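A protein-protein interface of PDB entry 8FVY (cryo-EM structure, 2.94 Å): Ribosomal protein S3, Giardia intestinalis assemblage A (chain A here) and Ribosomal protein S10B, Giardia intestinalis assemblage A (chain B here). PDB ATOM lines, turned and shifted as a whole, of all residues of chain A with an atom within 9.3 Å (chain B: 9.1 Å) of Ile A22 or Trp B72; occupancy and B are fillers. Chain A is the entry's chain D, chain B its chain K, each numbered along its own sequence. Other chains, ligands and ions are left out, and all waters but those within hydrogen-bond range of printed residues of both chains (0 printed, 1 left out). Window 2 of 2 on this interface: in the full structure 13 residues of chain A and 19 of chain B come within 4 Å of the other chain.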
ATOM      1  N   TYR A  14      29.280 -26.648   7.505  1.00  0.00           N
ATOM      2  CA  TYR A  14      29.105 -26.356   6.095  1.00  0.00           C
ATOM      3  C   TYR A  14      27.693 -26.685   5.642  1.00  0.00           C
ATOM      4  O   TYR A  14      27.121 -25.982   4.806  1.00  0.00           O
ATOM      5  CB  TYR A  14      30.136 -27.111   5.284  1.00  0.00           C
ATOM      6  CG  TYR A  14      31.537 -26.584   5.436  1.00  0.00           C
ATOM      7  CD1 TYR A  14      31.817 -25.259   5.238  1.00  0.00           C
ATOM      8  CD2 TYR A  14      32.582 -27.418   5.763  1.00  0.00           C
ATOM      9  CE1 TYR A  14      33.081 -24.777   5.366  1.00  0.00           C
ATOM     10  CE2 TYR A  14      33.851 -26.943   5.892  1.00  0.00           C
ATOM     11  CZ  TYR A  14      34.094 -25.619   5.690  1.00  0.00           C
ATOM     12  OH  TYR A  14      35.368 -25.134   5.815  1.00  0.00           O
ATOM     13  N   SER A  15      27.108 -27.742   6.192  1.00  0.00           N
ATOM     14  CA  SER A  15      25.764 -28.134   5.820  1.00  0.00           C
ATOM     15  C   SER A  15      24.711 -27.362   6.583  1.00  0.00           C
ATOM     16  O   SER A  15      23.532 -27.425   6.229  1.00  0.00           O
ATOM     17  CB  SER A  15      25.583 -29.618   6.061  1.00  0.00           C
ATOM     18  OG  SER A  15      24.573 -30.141   5.220  1.00  0.00           O
ATOM     19  N   LYS A  16      25.106 -26.655   7.623  1.00  0.00           N
ATOM     20  CA  LYS A  16      24.197 -25.814   8.370  1.00  0.00           C
ATOM     21  C   LYS A  16      24.128 -24.409   7.810  1.00  0.00           C
ATOM     22  O   LYS A  16      23.376 -23.585   8.331  1.00  0.00           O
ATOM     23  CB  LYS A  16      24.625 -25.780   9.829  1.00  0.00           C
ATOM     24  CG  LYS A  16      23.538 -25.414  10.774  1.00  0.00           C
ATOM     25  CD  LYS A  16      24.049 -24.453  11.826  1.00  0.00           C
ATOM     26  CE  LYS A  16      22.912 -23.791  12.575  1.00  0.00           C
ATOM     27  NZ  LYS A  16      21.838 -23.295  11.678  1.00  0.00           N
ATOM     28  N   TYR A  17      24.915 -24.121   6.784  1.00  0.00           N
ATOM     29  CA  TYR A  17      24.862 -22.876   6.037  1.00  0.00           C
ATOM     30  C   TYR A  17      24.081 -23.054   4.755  1.00  0.00           C
ATOM     31  O   TYR A  17      23.289 -22.189   4.375  1.00  0.00           O
ATOM     32  CB  TYR A  17      26.275 -22.413   5.705  1.00  0.00           C
ATOM     33  CG  TYR A  17      26.403 -20.978   5.324  1.00  0.00           C
ATOM     34  CD1 TYR A  17      26.493 -19.996   6.279  1.00  0.00           C
ATOM     35  CD2 TYR A  17      26.467 -20.606   4.008  1.00  0.00           C
ATOM     36  CE1 TYR A  17      26.617 -18.688   5.930  1.00  0.00           C
ATOM     37  CE2 TYR A  17      26.592 -19.307   3.655  1.00  0.00           C
ATOM     38  CZ  TYR A  17      26.667 -18.350   4.617  1.00  0.00           C
ATOM     39  OH  TYR A  17      26.791 -17.038   4.264  1.00  0.00           O
ATOM     40  N   LEU A  18      24.298 -24.185   4.098  1.00  0.00           N
ATOM     41  CA  LEU A  18      23.625 -24.483   2.849  1.00  0.00           C
ATOM     42  C   LEU A  18      22.122 -24.558   3.025  1.00  0.00           C
ATOM     43  O   LEU A  18      21.363 -24.001   2.226  1.00  0.00           O
ATOM     44  CB  LEU A  18      24.142 -25.805   2.322  1.00  0.00           C
ATOM     45  CG  LEU A  18      23.848 -26.129   0.873  1.00  0.00           C
ATOM     46  CD1 LEU A  18      24.572 -25.197  -0.035  1.00  0.00           C
ATOM     47  CD2 LEU A  18      24.217 -27.547   0.598  1.00  0.00           C
ATOM     48  N   ASN A  19      21.674 -25.256   4.059  1.00  0.00           N
ATOM     49  CA  ASN A  19      20.249 -25.419   4.290  1.00  0.00           C
ATOM     50  C   ASN A  19      19.567 -24.079   4.439  1.00  0.00           C
ATOM     51  O   ASN A  19      18.463 -23.865   3.929  1.00  0.00           O
ATOM     52  CB  ASN A  19      20.037 -26.250   5.538  1.00  0.00           C
ATOM     53  CG  ASN A  19      20.681 -27.597   5.446  1.00  0.00           C
ATOM     54  OD1 ASN A  19      21.395 -27.894   4.492  1.00  0.00           O
ATOM     55  ND2 ASN A  19      20.433 -28.428   6.436  1.00  0.00           N
ATOM     56  N   ASP A  20      20.208 -23.170   5.150  1.00  0.00           N
ATOM     57  CA  ASP A  20      19.632 -21.873   5.424  1.00  0.00           C
ATOM     58  C   ASP A  20      19.665 -20.956   4.216  1.00  0.00           C
ATOM     59  O   ASP A  20      18.811 -20.073   4.092  1.00  0.00           O
ATOM     60  CB  ASP A  20      20.363 -21.279   6.607  1.00  0.00           C
ATOM     61  CG  ASP A  20      20.133 -22.073   7.860  1.00  0.00           C
ATOM     62  OD1 ASP A  20      20.172 -23.316   7.776  1.00  0.00           O
ATOM     63  OD2 ASP A  20      19.898 -21.468   8.923  1.00  0.00           O
ATOM     64  N   CYS A  21      20.636 -21.138   3.332  1.00  0.00           N
ATOM     65  CA  CYS A  21      20.617 -20.414   2.073  1.00  0.00           C
ATOM     66  C   CYS A  21      19.438 -20.843   1.220  1.00  0.00           C
ATOM     67  O   CYS A  21      18.808 -20.017   0.552  1.00  0.00           O
ATOM     68  CB  CYS A  21      21.924 -20.633   1.335  1.00  0.00           C
ATOM     69  SG  CYS A  21      23.319 -19.729   2.000  1.00  0.00           S
ATOM     70  N   ILE A  22      19.132 -22.136   1.222  1.00  0.00           N
ATOM     71  CA  ILE A  22      17.971 -22.640   0.507  1.00  0.00           C
ATOM     72  C   ILE A  22      16.685 -22.138   1.135  1.00  0.00           C
ATOM     73  O   ILE A  22      15.759 -21.712   0.438  1.00  0.00           O
ATOM     74  CB  ILE A  22      18.012 -24.168   0.481  1.00  0.00           C
ATOM     75  CG1 ILE A  22      19.154 -24.636  -0.395  1.00  0.00           C
ATOM     76  CG2 ILE A  22      16.738 -24.698  -0.016  1.00  0.00           C
ATOM     77  CD1 ILE A  22      19.576 -26.016  -0.142  1.00  0.00           C
ATOM     78  N   MET A  23      16.601 -22.191   2.457  1.00  0.00           N
ATOM     79  CA  MET A  23      15.415 -21.713   3.147  1.00  0.00           C
ATOM     80  C   MET A  23      15.076 -20.292   2.740  1.00  0.00           C
ATOM     81  O   MET A  23      13.905 -19.908   2.735  1.00  0.00           O
ATOM     82  CB  MET A  23      15.653 -21.801   4.649  1.00  0.00           C
ATOM     83  CG  MET A  23      14.492 -21.418   5.520  1.00  0.00           C
ATOM     84  SD  MET A  23      15.013 -20.722   7.092  1.00  0.00           S
ATOM     85  CE  MET A  23      15.975 -22.082   7.734  1.00  0.00           C
ATOM     86  N   GLU A  24      16.086 -19.506   2.390  1.00  0.00           N
ATOM     87  CA  GLU A  24      15.874 -18.123   1.992  1.00  0.00           C
ATOM     88  C   GLU A  24      15.178 -18.020   0.646  1.00  0.00           C
ATOM     89  O   GLU A  24      14.374 -17.111   0.421  1.00  0.00           O
ATOM     90  CB  GLU A  24      17.217 -17.424   1.941  1.00  0.00           C
ATOM     91  CG  GLU A  24      17.169 -15.976   2.272  1.00  0.00           C
ATOM     92  CD  GLU A  24      18.346 -15.219   1.711  1.00  0.00           C
ATOM     93  OE1 GLU A  24      18.132 -14.170   1.071  1.00  0.00           O
ATOM     94  OE2 GLU A  24      19.489 -15.674   1.913  1.00  0.00           O
ATOM     95  N   ALA A  25      15.501 -18.924  -0.269  1.00  0.00           N
ATOM     96  CA  ALA A  25      14.964 -18.849  -1.614  1.00  0.00           C
ATOM     97  C   ALA A  25      13.482 -19.166  -1.648  1.00  0.00           C
ATOM     98  O   ALA A  25      12.713 -18.541  -2.392  1.00  0.00           O
ATOM     99  CB  ALA A  25      15.728 -19.808  -2.494  1.00  0.00           C
ATOM    100  N   GLU A  26      13.066 -20.155  -0.869  1.00  0.00           N
ATOM    101  CA  GLU A  26      11.653 -20.459  -0.773  1.00  0.00           C
ATOM    102  C   GLU A  26      10.877 -19.246  -0.299  1.00  0.00           C
ATOM    103  O   GLU A  26       9.761 -18.988  -0.760  1.00  0.00           O
ATOM    104  CB  GLU A  26      11.457 -21.637   0.160  1.00  0.00           C
ATOM    105  CG  GLU A  26      10.074 -22.195   0.134  1.00  0.00           C
ATOM    106  CD  GLU A  26       9.985 -23.582   0.707  1.00  0.00           C
ATOM    107  OE1 GLU A  26      10.958 -24.025   1.347  1.00  0.00           O
ATOM    108  OE2 GLU A  26       8.938 -24.232   0.516  1.00  0.00           O
ATOM    109  N   LEU A  27      11.467 -18.471   0.599  1.00  0.00           N
ATOM    110  CA  LEU A  27      10.818 -17.266   1.078  1.00  0.00           C
ATOM    111  C   LEU A  27      10.733 -16.220  -0.013  1.00  0.00           C
ATOM    112  O   LEU A  27       9.735 -15.508  -0.123  1.00  0.00           O
ATOM    113  CB  LEU A  27      11.583 -16.722   2.263  1.00  0.00           C
ATOM    114  CG  LEU A  27      11.614 -17.636   3.475  1.00  0.00           C
ATOM    115  CD1 LEU A  27      12.567 -17.117   4.474  1.00  0.00           C
ATOM    116  CD2 LEU A  27      10.256 -17.760   4.077  1.00  0.00           C
ATOM    117  N   HIS A  28      11.787 -16.090  -0.808  1.00  0.00           N
ATOM    118  CA  HIS A  28      11.753 -15.171  -1.934  1.00  0.00           C
ATOM    119  C   HIS A  28      10.581 -15.495  -2.834  1.00  0.00           C
ATOM    120  O   HIS A  28       9.779 -14.621  -3.180  1.00  0.00           O
ATOM    121  CB  HIS A  28      13.067 -15.266  -2.694  1.00  0.00           C
ATOM    122  CG  HIS A  28      13.208 -14.291  -3.815  1.00  0.00           C
ATOM    123  ND1 HIS A  28      13.365 -12.941  -3.607  1.00  0.00           N
ATOM    124  CD2 HIS A  28      13.274 -14.476  -5.152  1.00  0.00           C
ATOM    125  CE1 HIS A  28      13.486 -12.331  -4.771  1.00  0.00           C
ATOM    126  NE2 HIS A  28      13.435 -13.240  -5.725  1.00  0.00           N
ATOM    127  N   GLU A  29      10.438 -16.767  -3.174  1.00  0.00           N
ATOM    128  CA  GLU A  29       9.338 -17.187  -4.025  1.00  0.00           C
ATOM    129  C   GLU A  29       7.992 -16.903  -3.375  1.00  0.00           C
ATOM    130  O   GLU A  29       7.069 -16.397  -4.023  1.00  0.00           O
ATOM    131  CB  GLU A  29       9.500 -18.665  -4.328  1.00  0.00           C
ATOM    132  CG  GLU A  29       8.300 -19.373  -4.824  1.00  0.00           C
ATOM    133  CD  GLU A  29       7.879 -18.910  -6.206  1.00  0.00           C
ATOM    134  OE1 GLU A  29       8.514 -17.979  -6.744  1.00  0.00           O
ATOM    135  OE2 GLU A  29       6.924 -19.485  -6.767  1.00  0.00           O
ATOM    136  N   PHE A  30       7.866 -17.212  -2.092  1.00  0.00           N
ATOM    137  CA  PHE A  30       6.584 -17.084  -1.422  1.00  0.00           C
ATOM    138  C   PHE A  30       6.163 -15.629  -1.320  1.00  0.00           C
ATOM    139  O   PHE A  30       5.023 -15.272  -1.635  1.00  0.00           O
ATOM    140  CB  PHE A  30       6.690 -17.728  -0.051  1.00  0.00           C
ATOM    141  CG  PHE A  30       5.616 -17.345   0.890  1.00  0.00           C
ATOM    142  CD1 PHE A  30       4.347 -17.843   0.756  1.00  0.00           C
ATOM    143  CD2 PHE A  30       5.890 -16.519   1.937  1.00  0.00           C
ATOM    144  CE1 PHE A  30       3.373 -17.496   1.639  1.00  0.00           C
ATOM    145  CE2 PHE A  30       4.921 -16.176   2.813  1.00  0.00           C
ATOM    146  CZ  PHE A  30       3.663 -16.662   2.666  1.00  0.00           C
ATOM    147  N   ARG A  33       5.094 -14.318  -4.606  1.00  0.00           N
ATOM    148  CA  ARG A  33       3.745 -14.751  -4.913  1.00  0.00           C
ATOM    149  C   ARG A  33       2.717 -14.153  -3.974  1.00  0.00           C
ATOM    150  O   ARG A  33       1.518 -14.339  -4.194  1.00  0.00           O
ATOM    151  CB  ARG A  33       3.650 -16.271  -4.850  1.00  0.00           C
ATOM    152  CG  ARG A  33       4.178 -16.995  -6.056  1.00  0.00           C
ATOM    153  CD  ARG A  33       3.610 -18.377  -6.116  1.00  0.00           C
ATOM    154  NE  ARG A  33       4.587 -19.354  -6.579  1.00  0.00           N
ATOM    155  CZ  ARG A  33       4.295 -20.440  -7.281  1.00  0.00           C
ATOM    156  NH1 ARG A  33       3.070 -20.687  -7.707  1.00  0.00           N
ATOM    157  NH2 ARG A  33       5.258 -21.311  -7.556  1.00  0.00           N
ATOM    158  N   CYS A  43      14.745 -10.093   0.121  1.00  0.00           N
ATOM    159  CA  CYS A  43      14.699 -10.629   1.470  1.00  0.00           C
ATOM    160  C   CYS A  43      16.119 -10.888   1.939  1.00  0.00           C
ATOM    161  O   CYS A  43      17.071 -10.865   1.158  1.00  0.00           O
ATOM    162  CB  CYS A  43      13.892 -11.921   1.548  1.00  0.00           C
ATOM    163  SG  CYS A  43      14.836 -13.364   1.135  1.00  0.00           S
ATOM    164  N   LEU A  45      18.187 -12.870   5.723  1.00  0.00           N
ATOM    165  CA  LEU A  45      17.987 -13.707   6.889  1.00  0.00           C
ATOM    166  C   LEU A  45      19.184 -13.605   7.822  1.00  0.00           C
ATOM    167  O   LEU A  45      20.283 -13.225   7.419  1.00  0.00           O
ATOM    168  CB  LEU A  45      17.741 -15.147   6.463  1.00  0.00           C
ATOM    169  CG  LEU A  45      17.773 -16.241   7.515  1.00  0.00           C
ATOM    170  CD1 LEU A  45      16.772 -17.302   7.151  1.00  0.00           C
ATOM    171  CD2 LEU A  45      19.145 -16.835   7.595  1.00  0.00           C
ATOM    172  N   ARG A  82       6.114 -24.265   9.125  1.00  0.00           N
ATOM    173  CA  ARG A  82       6.717 -24.896   7.965  1.00  0.00           C
ATOM    174  C   ARG A  82       8.179 -25.210   8.211  1.00  0.00           C
ATOM    175  O   ARG A  82       8.646 -26.309   7.899  1.00  0.00           O
ATOM    176  CB  ARG A  82       6.555 -23.995   6.756  1.00  0.00           C
ATOM    177  CG  ARG A  82       6.980 -24.635   5.459  1.00  0.00           C
ATOM    178  CD  ARG A  82       8.340 -24.222   5.064  1.00  0.00           C
ATOM    179  NE  ARG A  82       8.951 -25.145   4.125  1.00  0.00           N
ATOM    180  CZ  ARG A  82       9.562 -26.261   4.482  1.00  0.00           C
ATOM    181  NH1 ARG A  82       9.485 -26.727   5.712  1.00  0.00           N
ATOM    182  NH2 ARG A  82      10.269 -26.926   3.582  1.00  0.00           N
ATOM    183  N   PHE A  83       8.922 -24.263   8.761  1.00  0.00           N
ATOM    184  CA  PHE A  83      10.320 -24.483   9.074  1.00  0.00           C
ATOM    185  C   PHE A  83      10.503 -25.022  10.473  1.00  0.00           C
ATOM    186  O   PHE A  83      11.638 -25.238  10.904  1.00  0.00           O
ATOM    187  CB  PHE A  83      11.103 -23.193   8.899  1.00  0.00           C
ATOM    188  CG  PHE A  83      11.088 -22.680   7.499  1.00  0.00           C
ATOM    189  CD1 PHE A  83      11.452 -23.499   6.453  1.00  0.00           C
ATOM    190  CD2 PHE A  83      10.685 -21.394   7.220  1.00  0.00           C
ATOM    191  CE1 PHE A  83      11.419 -23.043   5.164  1.00  0.00           C
ATOM    192  CE2 PHE A  83      10.656 -20.938   5.930  1.00  0.00           C
ATOM    193  CZ  PHE A  83      11.024 -21.762   4.903  1.00  0.00           C
ATOM    194  N   LEU B  24       1.308 -26.793   4.810  1.00  0.00           N
ATOM    195  CA  LEU B  24       1.069 -28.211   4.645  1.00  0.00           C
ATOM    196  C   LEU B  24       1.765 -28.718   3.396  1.00  0.00           C
ATOM    197  O   LEU B  24       1.848 -28.011   2.391  1.00  0.00           O
ATOM    198  CB  LEU B  24      -0.420 -28.465   4.574  1.00  0.00           C
ATOM    199  CG  LEU B  24      -0.893 -29.843   4.213  1.00  0.00           C
ATOM    200  CD1 LEU B  24      -0.882 -30.620   5.447  1.00  0.00           C
ATOM    201  CD2 LEU B  24      -2.259 -29.772   3.632  1.00  0.00           C
ATOM    202  N   LYS B  25       2.272 -29.935   3.481  1.00  0.00           N
ATOM    203  CA  LYS B  25       2.934 -30.572   2.359  1.00  0.00           C
ATOM    204  C   LYS B  25       1.951 -30.977   1.279  1.00  0.00           C
ATOM    205  O   LYS B  25       0.764 -31.177   1.531  1.00  0.00           O
ATOM    206  CB  LYS B  25       3.682 -31.801   2.833  1.00  0.00           C
ATOM    207  CG  LYS B  25       4.767 -32.301   1.922  1.00  0.00           C
ATOM    208  CD  LYS B  25       5.794 -31.276   1.644  1.00  0.00           C
ATOM    209  CE  LYS B  25       6.289 -30.619   2.908  1.00  0.00           C
ATOM    210  NZ  LYS B  25       7.519 -29.806   2.700  1.00  0.00           N
ATOM    211  N   GLU B  26       2.470 -31.111   0.071  1.00  0.00           N
ATOM    212  CA  GLU B  26       1.729 -31.656  -1.053  1.00  0.00           C
ATOM    213  C   GLU B  26       2.042 -33.140  -1.104  1.00  0.00           C
ATOM    214  O   GLU B  26       3.085 -33.550  -1.616  1.00  0.00           O
ATOM    215  CB  GLU B  26       2.125 -30.956  -2.341  1.00  0.00           C
ATOM    216  CG  GLU B  26       1.008 -30.729  -3.300  1.00  0.00           C
ATOM    217  CD  GLU B  26       0.279 -31.997  -3.676  1.00  0.00           C
ATOM    218  OE1 GLU B  26       0.909 -33.071  -3.673  1.00  0.00           O
ATOM    219  OE2 GLU B  26      -0.933 -31.916  -3.967  1.00  0.00           O
ATOM    220  N   THR B  69      -1.444 -20.083  -1.177  1.00  0.00           N
ATOM    221  CA  THR B  69      -0.315 -19.404  -1.785  1.00  0.00           C
ATOM    222  C   THR B  69       0.808 -20.400  -2.030  1.00  0.00           C
ATOM    223  O   THR B  69       1.912 -20.255  -1.504  1.00  0.00           O
ATOM    224  CB  THR B  69       0.151 -18.259  -0.900  1.00  0.00           C
ATOM    225  OG1 THR B  69      -0.952 -17.389  -0.625  1.00  0.00           O
ATOM    226  CG2 THR B  69       1.228 -17.503  -1.581  1.00  0.00           C
ATOM    227  N   PHE B  70       0.518 -21.412  -2.839  1.00  0.00           N
ATOM    228  CA  PHE B  70       1.456 -22.488  -3.121  1.00  0.00           C
ATOM    229  C   PHE B  70       2.845 -21.983  -3.462  1.00  0.00           C
ATOM    230  O   PHE B  70       3.032 -20.841  -3.879  1.00  0.00           O
ATOM    231  CB  PHE B  70       0.942 -23.313  -4.274  1.00  0.00           C
ATOM    232  CG  PHE B  70       1.347 -24.728  -4.220  1.00  0.00           C
ATOM    233  CD1 PHE B  70       0.671 -25.619  -3.440  1.00  0.00           C
ATOM    234  CD2 PHE B  70       2.400 -25.170  -4.960  1.00  0.00           C
ATOM    235  CE1 PHE B  70       1.047 -26.920  -3.399  1.00  0.00           C
ATOM    236  CE2 PHE B  70       2.772 -26.456  -4.927  1.00  0.00           C
ATOM    237  CZ  PHE B  70       2.097 -27.342  -4.140  1.00  0.00           C
ATOM    238  N   ALA B  71       3.821 -22.865  -3.293  1.00  0.00           N
ATOM    239  CA  ALA B  71       5.211 -22.515  -3.492  1.00  0.00           C
ATOM    240  C   ALA B  71       6.065 -23.720  -3.854  1.00  0.00           C
ATOM    241  O   ALA B  71       5.687 -24.520  -4.710  1.00  0.00           O
ATOM    242  CB  ALA B  71       5.717 -21.851  -2.242  1.00  0.00           C
ATOM    243  N   TRP B  72       7.227 -23.863  -3.231  1.00  0.00           N
ATOM    244  CA  TRP B  72       8.089 -25.007  -3.499  1.00  0.00           C
ATOM    245  C   TRP B  72       7.401 -26.267  -2.986  1.00  0.00           C
ATOM    246  O   TRP B  72       7.790 -26.893  -1.999  1.00  0.00           O
ATOM    247  CB  TRP B  72       9.443 -24.837  -2.841  1.00  0.00           C
ATOM    248  CG  TRP B  72      10.337 -23.926  -3.470  1.00  0.00           C
ATOM    249  CD1 TRP B  72      10.035 -22.950  -4.333  1.00  0.00           C
ATOM    250  CD2 TRP B  72      11.732 -23.881  -3.273  1.00  0.00           C
ATOM    251  NE1 TRP B  72      11.163 -22.290  -4.704  1.00  0.00           N
ATOM    252  CE2 TRP B  72      12.225 -22.852  -4.057  1.00  0.00           C
ATOM    253  CE3 TRP B  72      12.615 -24.621  -2.504  1.00  0.00           C
ATOM    254  CZ2 TRP B  72      13.555 -22.542  -4.098  1.00  0.00           C
ATOM    255  CZ3 TRP B  72      13.925 -24.317  -2.547  1.00  0.00           C
ATOM    256  CH2 TRP B  72      14.395 -23.291  -3.333  1.00  0.00           C
ATOM    257  N   ARG B  73       6.347 -26.620  -3.692  1.00  0.00           N
ATOM    258  CA  ARG B  73       5.520 -27.767  -3.371  1.00  0.00           C
ATOM    259  C   ARG B  73       5.182 -27.825  -1.884  1.00  0.00           C
ATOM    260  O   ARG B  73       5.342 -28.840  -1.209  1.00  0.00           O
ATOM    261  CB  ARG B  73       6.179 -29.043  -3.862  1.00  0.00           C
ATOM    262  CG  ARG B  73       7.298 -29.558  -3.112  1.00  0.00           C
ATOM    263  CD  ARG B  73       7.799 -30.787  -3.819  1.00  0.00           C
ATOM    264  NE  ARG B  73       6.818 -31.857  -3.943  1.00  0.00           N
ATOM    265  CZ  ARG B  73       5.906 -31.949  -4.905  1.00  0.00           C
ATOM    266  NH1 ARG B  73       5.806 -31.045  -5.862  1.00  0.00           N
ATOM    267  NH2 ARG B  73       5.080 -32.984  -4.918  1.00  0.00           N
ATOM    268  N   HIS B  74       4.653 -26.711  -1.394  1.00  0.00           N
ATOM    269  CA  HIS B  74       4.121 -26.602  -0.055  1.00  0.00           C
ATOM    270  C   HIS B  74       2.864 -25.766  -0.123  1.00  0.00           C
ATOM    271  O   HIS B  74       2.795 -24.790  -0.867  1.00  0.00           O
ATOM    272  CB  HIS B  74       5.099 -25.932   0.882  1.00  0.00           C
ATOM    273  CG  HIS B  74       5.174 -26.565   2.218  1.00  0.00           C
ATOM    274  ND1 HIS B  74       4.326 -26.249   3.253  1.00  0.00           N
ATOM    275  CD2 HIS B  74       6.049 -27.462   2.705  1.00  0.00           C
ATOM    276  CE1 HIS B  74       4.649 -26.969   4.310  1.00  0.00           C
ATOM    277  NE2 HIS B  74       5.694 -27.713   4.001  1.00  0.00           N
ATOM    278  N   HIS B  75       1.874 -26.151   0.655  1.00  0.00           N
ATOM    279  CA  HIS B  75       0.636 -25.407   0.754  1.00  0.00           C
ATOM    280  C   HIS B  75       0.712 -24.436   1.906  1.00  0.00           C
ATOM    281  O   HIS B  75       1.006 -24.832   3.034  1.00  0.00           O
ATOM    282  CB  HIS B  75      -0.542 -26.324   0.976  1.00  0.00           C
ATOM    283  CG  HIS B  75      -1.175 -26.830  -0.273  1.00  0.00           C
ATOM    284  ND1 HIS B  75      -1.815 -26.004  -1.167  1.00  0.00           N
ATOM    285  CD2 HIS B  75      -1.323 -28.087  -0.748  1.00  0.00           C
ATOM    286  CE1 HIS B  75      -2.302 -26.728  -2.158  1.00  0.00           C
ATOM    287  NE2 HIS B  75      -2.020 -27.995  -1.925  1.00  0.00           N
ATOM    288  N   TYR B  76       0.416 -23.180   1.628  1.00  0.00           N
ATOM    289  CA  TYR B  76       0.416 -22.130   2.630  1.00  0.00           C
ATOM    290  C   TYR B  76      -0.961 -21.504   2.690  1.00  0.00           C
ATOM    291  O   TYR B  76      -1.345 -20.756   1.789  1.00  0.00           O
ATOM    292  CB  TYR B  76       1.441 -21.073   2.308  1.00  0.00           C
ATOM    293  CG  TYR B  76       2.852 -21.529   2.362  1.00  0.00           C
ATOM    294  CD1 TYR B  76       3.441 -21.850   3.551  1.00  0.00           C
ATOM    295  CD2 TYR B  76       3.612 -21.583   1.229  1.00  0.00           C
ATOM    296  CE1 TYR B  76       4.740 -22.243   3.601  1.00  0.00           C
ATOM    297  CE2 TYR B  76       4.898 -21.973   1.269  1.00  0.00           C
ATOM    298  CZ  TYR B  76       5.464 -22.299   2.450  1.00  0.00           C
ATOM    299  OH  TYR B  76       6.772 -22.682   2.454  1.00  0.00           O
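O of Phe B70 lies close to NE of Arg A33 (3.5 Å).
The side-chain hydroxyl of Tyr B76 lies within hydrogen-bond range of the side-chain carboxylate of Glu A26.
The backbone carbonyl oxygen (O) of Leu B24 is in hydrogen-bond range of a ring nitrogen (ND1) of His B74, 3.2 Å away.
A ring nitrogen (NE2) of His B74 lies close to the side-chain amino group of Lys B25, at 3.1 Å.
The backbone NH (N) of Thr B69 sits at hydrogen-bond distance from the backbone carbonyl oxygen (O) of Tyr B76, 3.0 Å away.
The guanidinium group (NE) of Arg A82 lies within salt-bridge range of the side-chain carboxylate (OE1) of Glu A26, 3.6 Å away.
The side-chain carboxylate (OE2) of Glu A29 is in salt-bridge range of the guanidinium group (NH2) of Arg A33.
CG2 of Ile A22 touches CZ3 of Trp B72 (3.8 Å).
Ala A25 touches Trp B72.
Trp B72 touches Glu A26.
Phe A30 touches Thr B69 (CE1 to CG2, 3.9 Å).
Phe A30 touches Tyr B76.
CE1 of His B74 touches CG of Arg A82, at 3.5 Å.
Arg A82 touches Tyr B76 (CD to OH, 3.4 Å).
No residue of chain B comes within 4 Å of Cys A21.
Of the printed residues of chain B, Glu A26 touches Trp B72 (3.4 Å) and Tyr B76 (3.3 Å).
Of the printed residues of chain B, Phe A30 touches Thr B69 and Tyr B76.
Printed residues of chain A within 4 Å of Thr B69: Phe A30 (3.9 Å).
Printed residues of chain A within 4 Å of His B74: Arg A82 (3.5 Å).
Printed residues of chain A that touch a printed residue of chain B: Ile A22, Ala A25, Glu A26, Phe A30, Arg A33 and Arg A82.
Hydrophobic or aromatic side chains of chain A within 4 Å of the printed part of chain B: Ile A22, Ala A25 and Phe A30.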
